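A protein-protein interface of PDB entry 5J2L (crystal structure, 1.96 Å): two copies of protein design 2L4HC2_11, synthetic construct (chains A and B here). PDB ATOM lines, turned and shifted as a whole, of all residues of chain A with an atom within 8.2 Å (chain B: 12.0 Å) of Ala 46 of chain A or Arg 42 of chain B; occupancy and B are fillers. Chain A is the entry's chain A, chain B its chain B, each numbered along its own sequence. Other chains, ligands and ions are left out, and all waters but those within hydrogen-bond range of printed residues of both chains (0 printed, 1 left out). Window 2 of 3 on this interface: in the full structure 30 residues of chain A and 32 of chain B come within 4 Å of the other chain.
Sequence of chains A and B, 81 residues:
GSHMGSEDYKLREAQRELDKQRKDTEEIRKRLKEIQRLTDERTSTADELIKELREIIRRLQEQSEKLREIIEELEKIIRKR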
ATOM      1  N   THR A  39     -17.227 -16.208 -27.788  1.00  0.00           N
ATOM      2  CA  THR A  39     -15.773 -16.135 -27.813  1.00  0.00           C
ATOM      3  C   THR A  39     -15.228 -17.270 -28.674  1.00  0.00           C
ATOM      4  O   THR A  39     -14.380 -17.053 -29.551  1.00  0.00           O
ATOM      5  CB  THR A  39     -15.187 -16.214 -26.374  1.00  0.00           C
ATOM      6  OG1 THR A  39     -15.662 -15.106 -25.602  1.00  0.00           O
ATOM      7  CG2 THR A  39     -13.667 -16.195 -26.400  1.00  0.00           C
ATOM      8  N   THR A  43     -17.436 -14.695 -33.113  1.00  0.00           N
ATOM      9  CA  THR A  43     -18.413 -13.871 -33.830  1.00  0.00           C
ATOM     10  C   THR A  43     -18.431 -12.417 -33.371  1.00  0.00           C
ATOM     11  O   THR A  43     -19.006 -11.564 -34.050  1.00  0.00           O
ATOM     12  CB  THR A  43     -19.838 -14.455 -33.721  1.00  0.00           C
ATOM     13  OG1 THR A  43     -20.248 -14.472 -32.349  1.00  0.00           O
ATOM     14  CG2 THR A  43     -19.872 -15.870 -34.268  1.00  0.00           C
ATOM     15  N   SER A  44     -17.804 -12.127 -32.232  1.00  0.00           N
ATOM     16  CA  SER A  44     -17.797 -10.761 -31.714  1.00  0.00           C
ATOM     17  C   SER A  44     -16.400 -10.196 -31.632  1.00  0.00           C
ATOM     18  O   SER A  44     -15.417 -10.934 -31.574  1.00  0.00           O
ATOM     19  CB  SER A  44     -18.461 -10.687 -30.354  1.00  0.00           C
ATOM     20  OG  SER A  44     -19.823 -11.013 -30.441  1.00  0.00           O
ATOM     21  N   THR A  45     -16.315  -8.872 -31.633  1.00  0.00           N
ATOM     22  CA  THR A  45     -15.029  -8.210 -31.501  1.00  0.00           C
ATOM     23  C   THR A  45     -14.606  -8.308 -30.052  1.00  0.00           C
ATOM     24  O   THR A  45     -15.435  -8.557 -29.174  1.00  0.00           O
ATOM     25  CB  THR A  45     -15.060  -6.725 -31.919  1.00  0.00           C
ATOM     26  OG1 THR A  45     -15.909  -5.990 -31.027  1.00  0.00           O
ATOM     27  CG2 THR A  45     -15.595  -6.586 -33.334  1.00  0.00           C
ATOM     28  N   ALA A  46     -13.328  -8.096 -29.808  1.00  0.00           N
ATOM     29  CA  ALA A  46     -12.812  -8.123 -28.458  1.00  0.00           C
ATOM     30  C   ALA A  46     -13.522  -7.063 -27.630  1.00  0.00           C
ATOM     31  O   ALA A  46     -13.837  -7.292 -26.469  1.00  0.00           O
ATOM     32  CB  ALA A  46     -11.312  -7.916 -28.442  1.00  0.00           C
ATOM     33  N   ASP A  47     -13.776  -5.909 -28.239  1.00  0.00           N
ATOM     34  CA  ASP A  47     -14.452  -4.813 -27.561  1.00  0.00           C
ATOM     35  C   ASP A  47     -15.852  -5.209 -27.150  1.00  0.00           C
ATOM     36  O   ASP A  47     -16.298  -4.879 -26.054  1.00  0.00           O
ATOM     37  CB  ASP A  47     -14.491  -3.574 -28.445  1.00  0.00           C
ATOM     38  CG  ASP A  47     -13.127  -2.926 -28.583  1.00  0.00           C
ATOM     39  OD1 ASP A  47     -12.291  -3.185 -27.755  1.00  0.00           O
ATOM     40  OD2 ASP A  47     -12.918  -2.201 -29.528  1.00  0.00           O
ATOM     41  N   GLU A  48     -16.542  -5.913 -28.034  1.00  0.00           N
ATOM     42  CA  GLU A  48     -17.891  -6.369 -27.768  1.00  0.00           C
ATOM     43  C   GLU A  48     -17.893  -7.349 -26.608  1.00  0.00           C
ATOM     44  O   GLU A  48     -18.764  -7.292 -25.731  1.00  0.00           O
ATOM     45  CB  GLU A  48     -18.475  -6.987 -29.035  1.00  0.00           C
ATOM     46  CG  GLU A  48     -18.733  -5.956 -30.139  1.00  0.00           C
ATOM     47  CD  GLU A  48     -19.081  -6.559 -31.477  1.00  0.00           C
ATOM     48  OE1 GLU A  48     -18.894  -7.740 -31.652  1.00  0.00           O
ATOM     49  OE2 GLU A  48     -19.513  -5.824 -32.337  1.00  0.00           O
ATOM     50  N   LEU A  49     -16.898  -8.237 -26.606  1.00  0.00           N
ATOM     51  CA  LEU A  49     -16.781  -9.247 -25.567  1.00  0.00           C
ATOM     52  C   LEU A  49     -16.454  -8.598 -24.229  1.00  0.00           C
ATOM     53  O   LEU A  49     -17.018  -8.979 -23.202  1.00  0.00           O
ATOM     54  CB  LEU A  49     -15.721 -10.284 -25.958  1.00  0.00           C
ATOM     55  CG  LEU A  49     -16.104 -11.183 -27.150  1.00  0.00           C
ATOM     56  CD1 LEU A  49     -14.914 -12.043 -27.563  1.00  0.00           C
ATOM     57  CD2 LEU A  49     -17.288 -12.051 -26.751  1.00  0.00           C
ATOM     58  N   ILE A  50     -15.577  -7.605 -24.252  1.00  0.00           N
ATOM     59  CA  ILE A  50     -15.209  -6.883 -23.054  1.00  0.00           C
ATOM     60  C   ILE A  50     -16.416  -6.203 -22.451  1.00  0.00           C
ATOM     61  O   ILE A  50     -16.589  -6.199 -21.232  1.00  0.00           O
ATOM     62  CB  ILE A  50     -14.095  -5.870 -23.322  1.00  0.00           C
ATOM     63  CG1 ILE A  50     -12.790  -6.607 -23.636  1.00  0.00           C
ATOM     64  CG2 ILE A  50     -13.942  -4.944 -22.132  1.00  0.00           C
ATOM     65  CD1 ILE A  50     -11.706  -5.712 -24.193  1.00  0.00           C
ATOM     66  N   LYS A  51     -17.252  -5.620 -23.307  1.00  0.00           N
ATOM     67  CA  LYS A  51     -18.438  -4.924 -22.827  1.00  0.00           C
ATOM     68  C   LYS A  51     -19.335  -5.881 -22.046  1.00  0.00           C
ATOM     69  O   LYS A  51     -19.757  -5.571 -20.923  1.00  0.00           O
ATOM     70  CB  LYS A  51     -19.184  -4.296 -24.003  1.00  0.00           C
ATOM     71  CG  LYS A  51     -18.440  -3.122 -24.625  1.00  0.00           C
ATOM     72  CD  LYS A  51     -19.173  -2.548 -25.834  1.00  0.00           C
ATOM     73  CE  LYS A  51     -18.361  -1.434 -26.484  1.00  0.00           C
ATOM     74  NZ  LYS A  51     -19.046  -0.866 -27.679  1.00  0.00           N
ATOM     75  N   GLU A  52     -19.593  -7.055 -22.621  1.00  0.00           N
ATOM     76  CA  GLU A  52     -20.432  -8.016 -21.940  1.00  0.00           C
ATOM     77  C   GLU A  52     -19.793  -8.541 -20.659  1.00  0.00           C
ATOM     78  O   GLU A  52     -20.499  -8.770 -19.676  1.00  0.00           O
ATOM     79  CB  GLU A  52     -20.852  -9.157 -22.862  1.00  0.00           C
ATOM     80  CG  GLU A  52     -21.909  -8.738 -23.886  1.00  0.00           C
ATOM     81  CD  GLU A  52     -22.500  -9.888 -24.665  1.00  0.00           C
ATOM     82  OE1 GLU A  52     -21.807 -10.848 -24.892  1.00  0.00           O
ATOM     83  OE2 GLU A  52     -23.670  -9.830 -24.985  1.00  0.00           O
ATOM     84  N   LEU A  53     -18.483  -8.716 -20.651  1.00  0.00           N
ATOM     85  CA  LEU A  53     -17.813  -9.197 -19.426  1.00  0.00           C
ATOM     86  C   LEU A  53     -17.850  -8.153 -18.302  1.00  0.00           C
ATOM     87  O   LEU A  53     -17.984  -8.507 -17.126  1.00  0.00           O
ATOM     88  CB  LEU A  53     -16.383  -9.621 -19.759  1.00  0.00           C
ATOM     89  CG  LEU A  53     -16.284 -10.873 -20.639  1.00  0.00           C
ATOM     90  CD1 LEU A  53     -14.841 -11.082 -21.065  1.00  0.00           C
ATOM     91  CD2 LEU A  53     -16.804 -12.078 -19.853  1.00  0.00           C
ATOM     92  N   ARG A  54     -17.743  -6.868 -18.655  1.00  0.00           N
ATOM     93  CA  ARG A  54     -17.845  -5.814 -17.643  1.00  0.00           C
ATOM     94  C   ARG A  54     -19.230  -5.791 -17.035  1.00  0.00           C
ATOM     95  O   ARG A  54     -19.378  -5.487 -15.852  1.00  0.00           O
ATOM     96  CB  ARG A  54     -17.482  -4.453 -18.204  1.00  0.00           C
ATOM     97  CG  ARG A  54     -16.000  -4.260 -18.433  1.00  0.00           C
ATOM     98  CD  ARG A  54     -15.685  -2.963 -19.087  1.00  0.00           C
ATOM     99  NE  ARG A  54     -14.250  -2.710 -19.099  1.00  0.00           N
ATOM    100  CZ  ARG A  54     -13.596  -1.960 -20.003  1.00  0.00           C
ATOM    101  NH1 ARG A  54     -14.242  -1.407 -21.007  1.00  0.00           N
ATOM    102  NH2 ARG A  54     -12.296  -1.774 -19.875  1.00  0.00           N
ATOM    103  N   LYS B  33     -12.913  -6.681  -8.201  1.00  0.00           N
ATOM    104  CA  LYS B  33     -12.179  -5.449  -8.528  1.00  0.00           C
ATOM    105  C   LYS B  33     -10.963  -5.762  -9.370  1.00  0.00           C
ATOM    106  O   LYS B  33     -10.683  -5.073 -10.354  1.00  0.00           O
ATOM    107  CB  LYS B  33     -11.735  -4.701  -7.265  1.00  0.00           C
ATOM    108  CG  LYS B  33     -12.841  -4.008  -6.509  1.00  0.00           C
ATOM    109  CD  LYS B  33     -12.308  -3.322  -5.245  1.00  0.00           C
ATOM    110  CE  LYS B  33     -11.427  -2.117  -5.588  1.00  0.00           C
ATOM    111  NZ  LYS B  33     -10.912  -1.418  -4.369  1.00  0.00           N
ATOM    112  N   GLU B  34     -10.244  -6.816  -8.983  1.00  0.00           N
ATOM    113  CA  GLU B  34      -9.049  -7.225  -9.699  1.00  0.00           C
ATOM    114  C   GLU B  34      -9.399  -7.616 -11.134  1.00  0.00           C
ATOM    115  O   GLU B  34      -8.708  -7.242 -12.088  1.00  0.00           O
ATOM    116  CB  GLU B  34      -8.353  -8.383  -8.957  1.00  0.00           C
ATOM    117  CG  GLU B  34      -7.723  -8.000  -7.625  1.00  0.00           C
ATOM    118  CD  GLU B  34      -7.203  -9.182  -6.819  1.00  0.00           C
ATOM    119  OE1 GLU B  34      -7.167 -10.277  -7.324  1.00  0.00           O
ATOM    120  OE2 GLU B  34      -6.872  -8.989  -5.673  1.00  0.00           O
ATOM    121  N   ILE B  35     -10.495  -8.351 -11.279  1.00  0.00           N
ATOM    122  CA  ILE B  35     -10.898  -8.850 -12.591  1.00  0.00           C
ATOM    123  C   ILE B  35     -11.278  -7.648 -13.467  1.00  0.00           C
ATOM    124  O   ILE B  35     -10.893  -7.583 -14.640  1.00  0.00           O
ATOM    125  CB  ILE B  35     -12.052  -9.865 -12.445  1.00  0.00           C
ATOM    126  CG1 ILE B  35     -11.528 -11.111 -11.714  1.00  0.00           C
ATOM    127  CG2 ILE B  35     -12.575 -10.271 -13.820  1.00  0.00           C
ATOM    128  CD1 ILE B  35     -12.625 -12.064 -11.245  1.00  0.00           C
ATOM    129  N   GLN B  36     -11.998  -6.700 -12.888  1.00  0.00           N
ATOM    130  CA  GLN B  36     -12.358  -5.467 -13.579  1.00  0.00           C
ATOM    131  C   GLN B  36     -11.108  -4.742 -14.087  1.00  0.00           C
ATOM    132  O   GLN B  36     -11.081  -4.261 -15.221  1.00  0.00           O
ATOM    133  CB  GLN B  36     -13.175  -4.573 -12.653  1.00  0.00           C
ATOM    134  CG  GLN B  36     -13.588  -3.239 -13.231  1.00  0.00           C
ATOM    135  CD  GLN B  36     -14.501  -3.343 -14.415  1.00  0.00           C
ATOM    136  OE1 GLN B  36     -15.543  -4.003 -14.381  1.00  0.00           O
ATOM    137  NE2 GLN B  36     -14.114  -2.661 -15.485  1.00  0.00           N
ATOM    138  N   ARG B  37     -10.073  -4.700 -13.257  1.00  0.00           N
ATOM    139  CA  ARG B  37      -8.834  -4.041 -13.631  1.00  0.00           C
ATOM    140  C   ARG B  37      -8.160  -4.756 -14.802  1.00  0.00           C
ATOM    141  O   ARG B  37      -7.617  -4.101 -15.694  1.00  0.00           O
ATOM    142  CB  ARG B  37      -7.870  -3.917 -12.441  1.00  0.00           C
ATOM    143  CG  ARG B  37      -8.332  -2.933 -11.361  1.00  0.00           C
ATOM    144  CD  ARG B  37      -7.206  -2.502 -10.481  1.00  0.00           C
ATOM    145  NE  ARG B  37      -6.724  -3.436  -9.486  1.00  0.00           N
ATOM    146  CZ  ARG B  37      -6.990  -3.398  -8.156  1.00  0.00           C
ATOM    147  NH1 ARG B  37      -7.748  -2.465  -7.616  1.00  0.00           N
ATOM    148  NH2 ARG B  37      -6.421  -4.293  -7.370  1.00  0.00           N
ATOM    149  N   LEU B  38      -8.206  -6.087 -14.817  1.00  0.00           N
ATOM    150  CA  LEU B  38      -7.646  -6.828 -15.945  1.00  0.00           C
ATOM    151  C   LEU B  38      -8.368  -6.497 -17.223  1.00  0.00           C
ATOM    152  O   LEU B  38      -7.751  -6.386 -18.287  1.00  0.00           O
ATOM    153  CB  LEU B  38      -7.711  -8.336 -15.729  1.00  0.00           C
ATOM    154  CG  LEU B  38      -6.759  -8.886 -14.698  1.00  0.00           C
ATOM    155  CD1 LEU B  38      -7.075 -10.354 -14.486  1.00  0.00           C
ATOM    156  CD2 LEU B  38      -5.332  -8.679 -15.207  1.00  0.00           C
ATOM    157  N   THR B  39      -9.677  -6.334 -17.118  1.00  0.00           N
ATOM    158  CA  THR B  39     -10.473  -5.991 -18.269  1.00  0.00           C
ATOM    159  C   THR B  39      -9.950  -4.700 -18.872  1.00  0.00           C
ATOM    160  O   THR B  39      -9.902  -4.552 -20.092  1.00  0.00           O
ATOM    161  CB  THR B  39     -11.963  -5.842 -17.921  1.00  0.00           C
ATOM    162  OG1 THR B  39     -12.482  -7.078 -17.409  1.00  0.00           O
ATOM    163  CG2 THR B  39     -12.726  -5.478 -19.153  1.00  0.00           C
ATOM    164  N   ASP B  40      -9.582  -3.760 -18.001  1.00  0.00           N
ATOM    165  CA  ASP B  40      -9.096  -2.445 -18.416  1.00  0.00           C
ATOM    166  C   ASP B  40      -7.707  -2.519 -19.047  1.00  0.00           C
ATOM    167  O   ASP B  40      -7.463  -1.905 -20.088  1.00  0.00           O
ATOM    168  CB  ASP B  40      -9.099  -1.482 -17.226  1.00  0.00           C
ATOM    169  CG  ASP B  40     -10.513  -1.181 -16.737  1.00  0.00           C
ATOM    170  OD1 ASP B  40     -11.450  -1.468 -17.451  1.00  0.00           O
ATOM    171  OD2 ASP B  40     -10.647  -0.686 -15.642  1.00  0.00           O
ATOM    172  N   GLU B  41      -6.797  -3.287 -18.442  1.00  0.00           N
ATOM    173  CA  GLU B  41      -5.461  -3.408 -19.021  1.00  0.00           C
ATOM    174  C   GLU B  41      -5.568  -3.907 -20.434  1.00  0.00           C
ATOM    175  O   GLU B  41      -4.852  -3.453 -21.326  1.00  0.00           O
ATOM    176  CB  GLU B  41      -4.563  -4.384 -18.268  1.00  0.00           C
ATOM    177  CG  GLU B  41      -4.082  -3.966 -16.902  1.00  0.00           C
ATOM    178  CD  GLU B  41      -3.198  -5.042 -16.340  1.00  0.00           C
ATOM    179  OE1 GLU B  41      -3.011  -6.029 -17.022  1.00  0.00           O
ATOM    180  OE2 GLU B  41      -2.700  -4.879 -15.249  1.00  0.00           O
ATOM    181  N   ARG B  42      -6.464  -4.861 -20.626  1.00  0.00           N
ATOM    182  CA  ARG B  42      -6.676  -5.466 -21.923  1.00  0.00           C
ATOM    183  C   ARG B  42      -5.399  -6.146 -22.395  1.00  0.00           C
ATOM    184  O   ARG B  42      -5.059  -6.143 -23.581  1.00  0.00           O
ATOM    185  CB  ARG B  42      -7.189  -4.450 -22.923  1.00  0.00           C
ATOM    186  CG  ARG B  42      -7.507  -5.031 -24.285  1.00  0.00           C
ATOM    187  CD  ARG B  42      -8.246  -4.068 -25.120  1.00  0.00           C
ATOM    188  NE  ARG B  42      -8.495  -4.591 -26.448  1.00  0.00           N
ATOM    189  CZ  ARG B  42      -9.363  -4.039 -27.316  1.00  0.00           C
ATOM    190  NH1 ARG B  42     -10.042  -2.972 -26.957  1.00  0.00           N
ATOM    191  NH2 ARG B  42      -9.543  -4.568 -28.517  1.00  0.00           N
ATOM    192  N   THR B  43      -4.708  -6.760 -21.444  1.00  0.00           N
ATOM    193  CA  THR B  43      -3.521  -7.546 -21.729  1.00  0.00           C
ATOM    194  C   THR B  43      -3.912  -9.031 -21.644  1.00  0.00           C
ATOM    195  O   THR B  43      -3.059  -9.914 -21.759  1.00  0.00           O
ATOM    196  CB  THR B  43      -2.349  -7.236 -20.738  1.00  0.00           C
ATOM    197  OG1 THR B  43      -2.733  -7.566 -19.386  1.00  0.00           O
ATOM    198  CG2 THR B  43      -1.957  -5.766 -20.801  1.00  0.00           C
ATOM    199  N   SER B  44      -5.208  -9.288 -21.414  1.00  0.00           N
ATOM    200  CA  SER B  44      -5.726 -10.642 -21.175  1.00  0.00           C
ATOM    201  C   SER B  44      -6.807 -11.041 -22.184  1.00  0.00           C
ATOM    202  O   SER B  44      -7.484 -10.187 -22.756  1.00  0.00           O
ATOM    203  CB  SER B  44      -6.285 -10.746 -19.755  1.00  0.00           C
ATOM    204  OG  SER B  44      -5.290 -10.526 -18.790  1.00  0.00           O
ATOM    205  N   THR B  45      -6.959 -12.349 -22.389  1.00  0.00           N
ATOM    206  CA  THR B  45      -7.961 -12.882 -23.310  1.00  0.00           C
ATOM    207  C   THR B  45      -9.322 -12.988 -22.660  1.00  0.00           C
ATOM    208  O   THR B  45      -9.433 -13.047 -21.437  1.00  0.00           O
ATOM    209  CB  THR B  45      -7.573 -14.272 -23.821  1.00  0.00           C
ATOM    210  OG1 THR B  45      -7.523 -15.174 -22.711  1.00  0.00           O
ATOM    211  CG2 THR B  45      -6.213 -14.227 -24.490  1.00  0.00           C
ATOM    212  N   ALA B  46     -10.353 -13.064 -23.487  1.00  0.00           N
ATOM    213  CA  ALA B  46     -11.682 -13.255 -22.971  1.00  0.00           C
ATOM    214  C   ALA B  46     -11.741 -14.619 -22.276  1.00  0.00           C
ATOM    215  O   ALA B  46     -12.331 -14.731 -21.210  1.00  0.00           O
ATOM    216  CB  ALA B  46     -12.721 -13.135 -24.067  1.00  0.00           C
ATOM    217  N   ASP B  47     -11.110 -15.658 -22.855  1.00  0.00           N
ATOM    218  CA  ASP B  47     -11.111 -16.980 -22.199  1.00  0.00           C
ATOM    219  C   ASP B  47     -10.599 -16.904 -20.770  1.00  0.00           C
ATOM    220  O   ASP B  47     -11.180 -17.516 -19.865  1.00  0.00           O
ATOM    221  CB  ASP B  47     -10.287 -18.024 -22.971  1.00  0.00           C
ATOM    222  CG  ASP B  47     -10.977 -18.618 -24.194  1.00  0.00           C
ATOM    223  OD1 ASP B  47     -12.179 -18.562 -24.266  1.00  0.00           O
ATOM    224  OD2 ASP B  47     -10.287 -19.139 -25.042  1.00  0.00           O
ATOM    225  N   GLU B  48      -9.501 -16.172 -20.579  1.00  0.00           N
ATOM    226  CA  GLU B  48      -8.904 -16.015 -19.262  1.00  0.00           C
ATOM    227  C   GLU B  48      -9.826 -15.268 -18.300  1.00  0.00           C
ATOM    228  O   GLU B  48      -9.932 -15.635 -17.130  1.00  0.00           O
ATOM    229  CB  GLU B  48      -7.563 -15.310 -19.385  1.00  0.00           C
ATOM    230  CG  GLU B  48      -6.475 -16.169 -20.009  1.00  0.00           C
ATOM    231  CD  GLU B  48      -5.210 -15.409 -20.301  1.00  0.00           C
ATOM    232  OE1 GLU B  48      -5.242 -14.549 -21.155  1.00  0.00           O
ATOM    233  OE2 GLU B  48      -4.217 -15.678 -19.660  1.00  0.00           O
ATOM    234  N   LEU B  49     -10.479 -14.222 -18.794  1.00  0.00           N
ATOM    235  CA  LEU B  49     -11.387 -13.429 -17.970  1.00  0.00           C
ATOM    236  C   LEU B  49     -12.601 -14.263 -17.588  1.00  0.00           C
ATOM    237  O   LEU B  49     -13.068 -14.221 -16.445  1.00  0.00           O
ATOM    238  CB  LEU B  49     -11.819 -12.194 -18.744  1.00  0.00           C
ATOM    239  CG  LEU B  49     -10.720 -11.168 -19.041  1.00  0.00           C
ATOM    240  CD1 LEU B  49     -11.269 -10.110 -19.985  1.00  0.00           C
ATOM    241  CD2 LEU B  49     -10.250 -10.548 -17.739  1.00  0.00           C
ATOM    242  N   ILE B  50     -13.097 -15.036 -18.555  1.00  0.00           N
ATOM    243  CA  ILE B  50     -14.246 -15.897 -18.343  1.00  0.00           C
ATOM    244  C   ILE B  50     -13.932 -16.950 -17.280  1.00  0.00           C
ATOM    245  O   ILE B  50     -14.769 -17.250 -16.425  1.00  0.00           O
ATOM    246  CB  ILE B  50     -14.707 -16.552 -19.657  1.00  0.00           C
ATOM    247  CG1 ILE B  50     -15.269 -15.480 -20.596  1.00  0.00           C
ATOM    248  CG2 ILE B  50     -15.765 -17.610 -19.375  1.00  0.00           C
ATOM    249  CD1 ILE B  50     -15.523 -15.969 -22.011  1.00  0.00           C
ATOM    250  N   GLU B  52     -11.839 -16.684 -14.794  1.00  0.00           N
ATOM    251  CA  GLU B  52     -11.818 -16.084 -13.467  1.00  0.00           C
ATOM    252  C   GLU B  52     -13.243 -15.796 -12.960  1.00  0.00           C
ATOM    253  O   GLU B  52     -13.526 -15.981 -11.776  1.00  0.00           O
ATOM    254  CB  GLU B  52     -10.914 -14.838 -13.449  1.00  0.00           C
ATOM    255  CG  GLU B  52      -9.431 -15.203 -13.625  1.00  0.00           C
ATOM    256  CD  GLU B  52      -8.431 -14.076 -13.455  1.00  0.00           C
ATOM    257  OE1 GLU B  52      -8.604 -13.256 -12.580  1.00  0.00           O
ATOM    258  OE2 GLU B  52      -7.466 -14.061 -14.192  1.00  0.00           O
ATOM    259  N   LEU B  53     -14.138 -15.376 -13.850  1.00  0.00           N
ATOM    260  CA  LEU B  53     -15.507 -15.089 -13.456  1.00  0.00           C
ATOM    261  C   LEU B  53     -16.273 -16.370 -13.102  1.00  0.00           C
ATOM    262  O   LEU B  53     -17.081 -16.374 -12.172  1.00  0.00           O
ATOM    263  CB  LEU B  53     -16.189 -14.285 -14.548  1.00  0.00           C
ATOM    264  CG  LEU B  53     -15.646 -12.860 -14.691  1.00  0.00           C
ATOM    265  CD1 LEU B  53     -16.233 -12.204 -15.934  1.00  0.00           C
ATOM    266  CD2 LEU B  53     -16.009 -12.066 -13.433  1.00  0.00           C
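Among the printed residues, pairs that only touch across the chains: Thr 39 of chain A with Ala 46 of chain B (3.9 Å), Thr 39 of chain A with Asp 47 of chain B (3.5 Å), Thr 39 of chain A with Ile 50 of chain B (3.7 Å), Ala 46 of chain A with Arg 42 of chain B (3.8 Å), Ile 50 of chain A with Thr 39 of chain B (3.3 Å), Ile 50 of chain A with Arg 42 of chain B (3.9 Å), Leu 53 of chain A with Leu 49 of chain B (3.9 Å), Leu 53 of chain A with Ile 50 of chain B (3.8 Å), Leu 53 of chain A with Leu 53 of chain B (3.96 Å), Arg 54 of chain A with Gln 36 of chain B (3.6 Å) and Arg 54 of chain A with Thr 39 of chain B (3.2 Å).
Ala 46 of chain A touches just one residue of chain B: Arg 42 (3.8 Å). Of chain A, only Ala 46 (3.8 Å), Asp 47 (2.4 Å) and Ile 50 (3.9 Å) come within 4 Å of Arg 42 of chain B. No residue of chain B comes within 4 Å of Ser 44 of chain A. No residue of chain B comes within 4 Å of Thr 45 of chain A. Asp 47 of chain A touches one residue of chain B. No residue of chain B comes within 4 Å of Glu 48 of chain A. Leu 49 of chain A touches none of the printed residues of chain B. Ile 50 of chain A touches just these residues of chain B: Thr 39 (3.3 Å) and Arg 42 (3.9 Å). Of the printed residues of chain B, Thr 39 of chain A touches Ala 46, Asp 47 and Ile 50. Of the printed residues of chain A, Gln 36 of chain B touches Arg 54. Of the printed residues of chain A, Ala 46 of chain B touches Thr 39. Of the printed residues of chain A, Leu 49 of chain B touches Leu 53. Printed residues of chain A within 4 Å of Leu 53 of chain B: Leu 53 (3.96 Å). Glu 52 of chain B touches none of the printed residues of chain A. The nearest residue of chain A that does not touch Arg 42 of chain B is Thr 45 of chain A (6.5 Å). The nearest printed residue of chain A that does not touch Leu 53 of chain B is Arg 54 of chain A (6.2 Å).
Among the printed residues, 13 pairs touch across the chains. Among the printed residues, Asp or Glu carboxylates within 4 Å of a Lys or Arg side-chain nitrogen of the other chain: Asp 47 of chain A with Arg 42 of chain B and Arg 54 of chain A with Asp 40 of chain B.
The side-chain hydroxyl of Thr 39 of chain B is in hydrogen-bond range of the backbone carbonyl oxygen of Ile 35 of chain B (3.2 Å).
Thr 39 of chain A touches Ala 46 of chain B, but with the chains exchanged Ala 46 of chain A does not touch Thr 39 of chain B (7.6 Å). Thr 39 of chain A touches Asp 47 of chain B, but with the chains exchanged Asp 47 of chain A does not touch Thr 39 of chain B (7.8 Å). Leu 53 of chain A touches Leu 49 of chain B, but with the chains exchanged Leu 49 of chain A does not touch Leu 53 of chain B (8.0 Å). Leu 53 of chain A touches its own counterpart, Leu 53 of chain B. Of the 13 pairs that touch across the chains among the printed residues, 3 have their exchanged pair printed and touching as well.
The guanidinium group of Arg 54 of chain A lies within salt-bridge range of the side-chain carboxylate of Asp 40 of chain B (2.6 Å). The guanidinium group (NH2) of Arg 42 of chain B lies within salt-bridge range of the side-chain carboxylate (OD1) of Asp 47 of chain A (3.2 Å).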
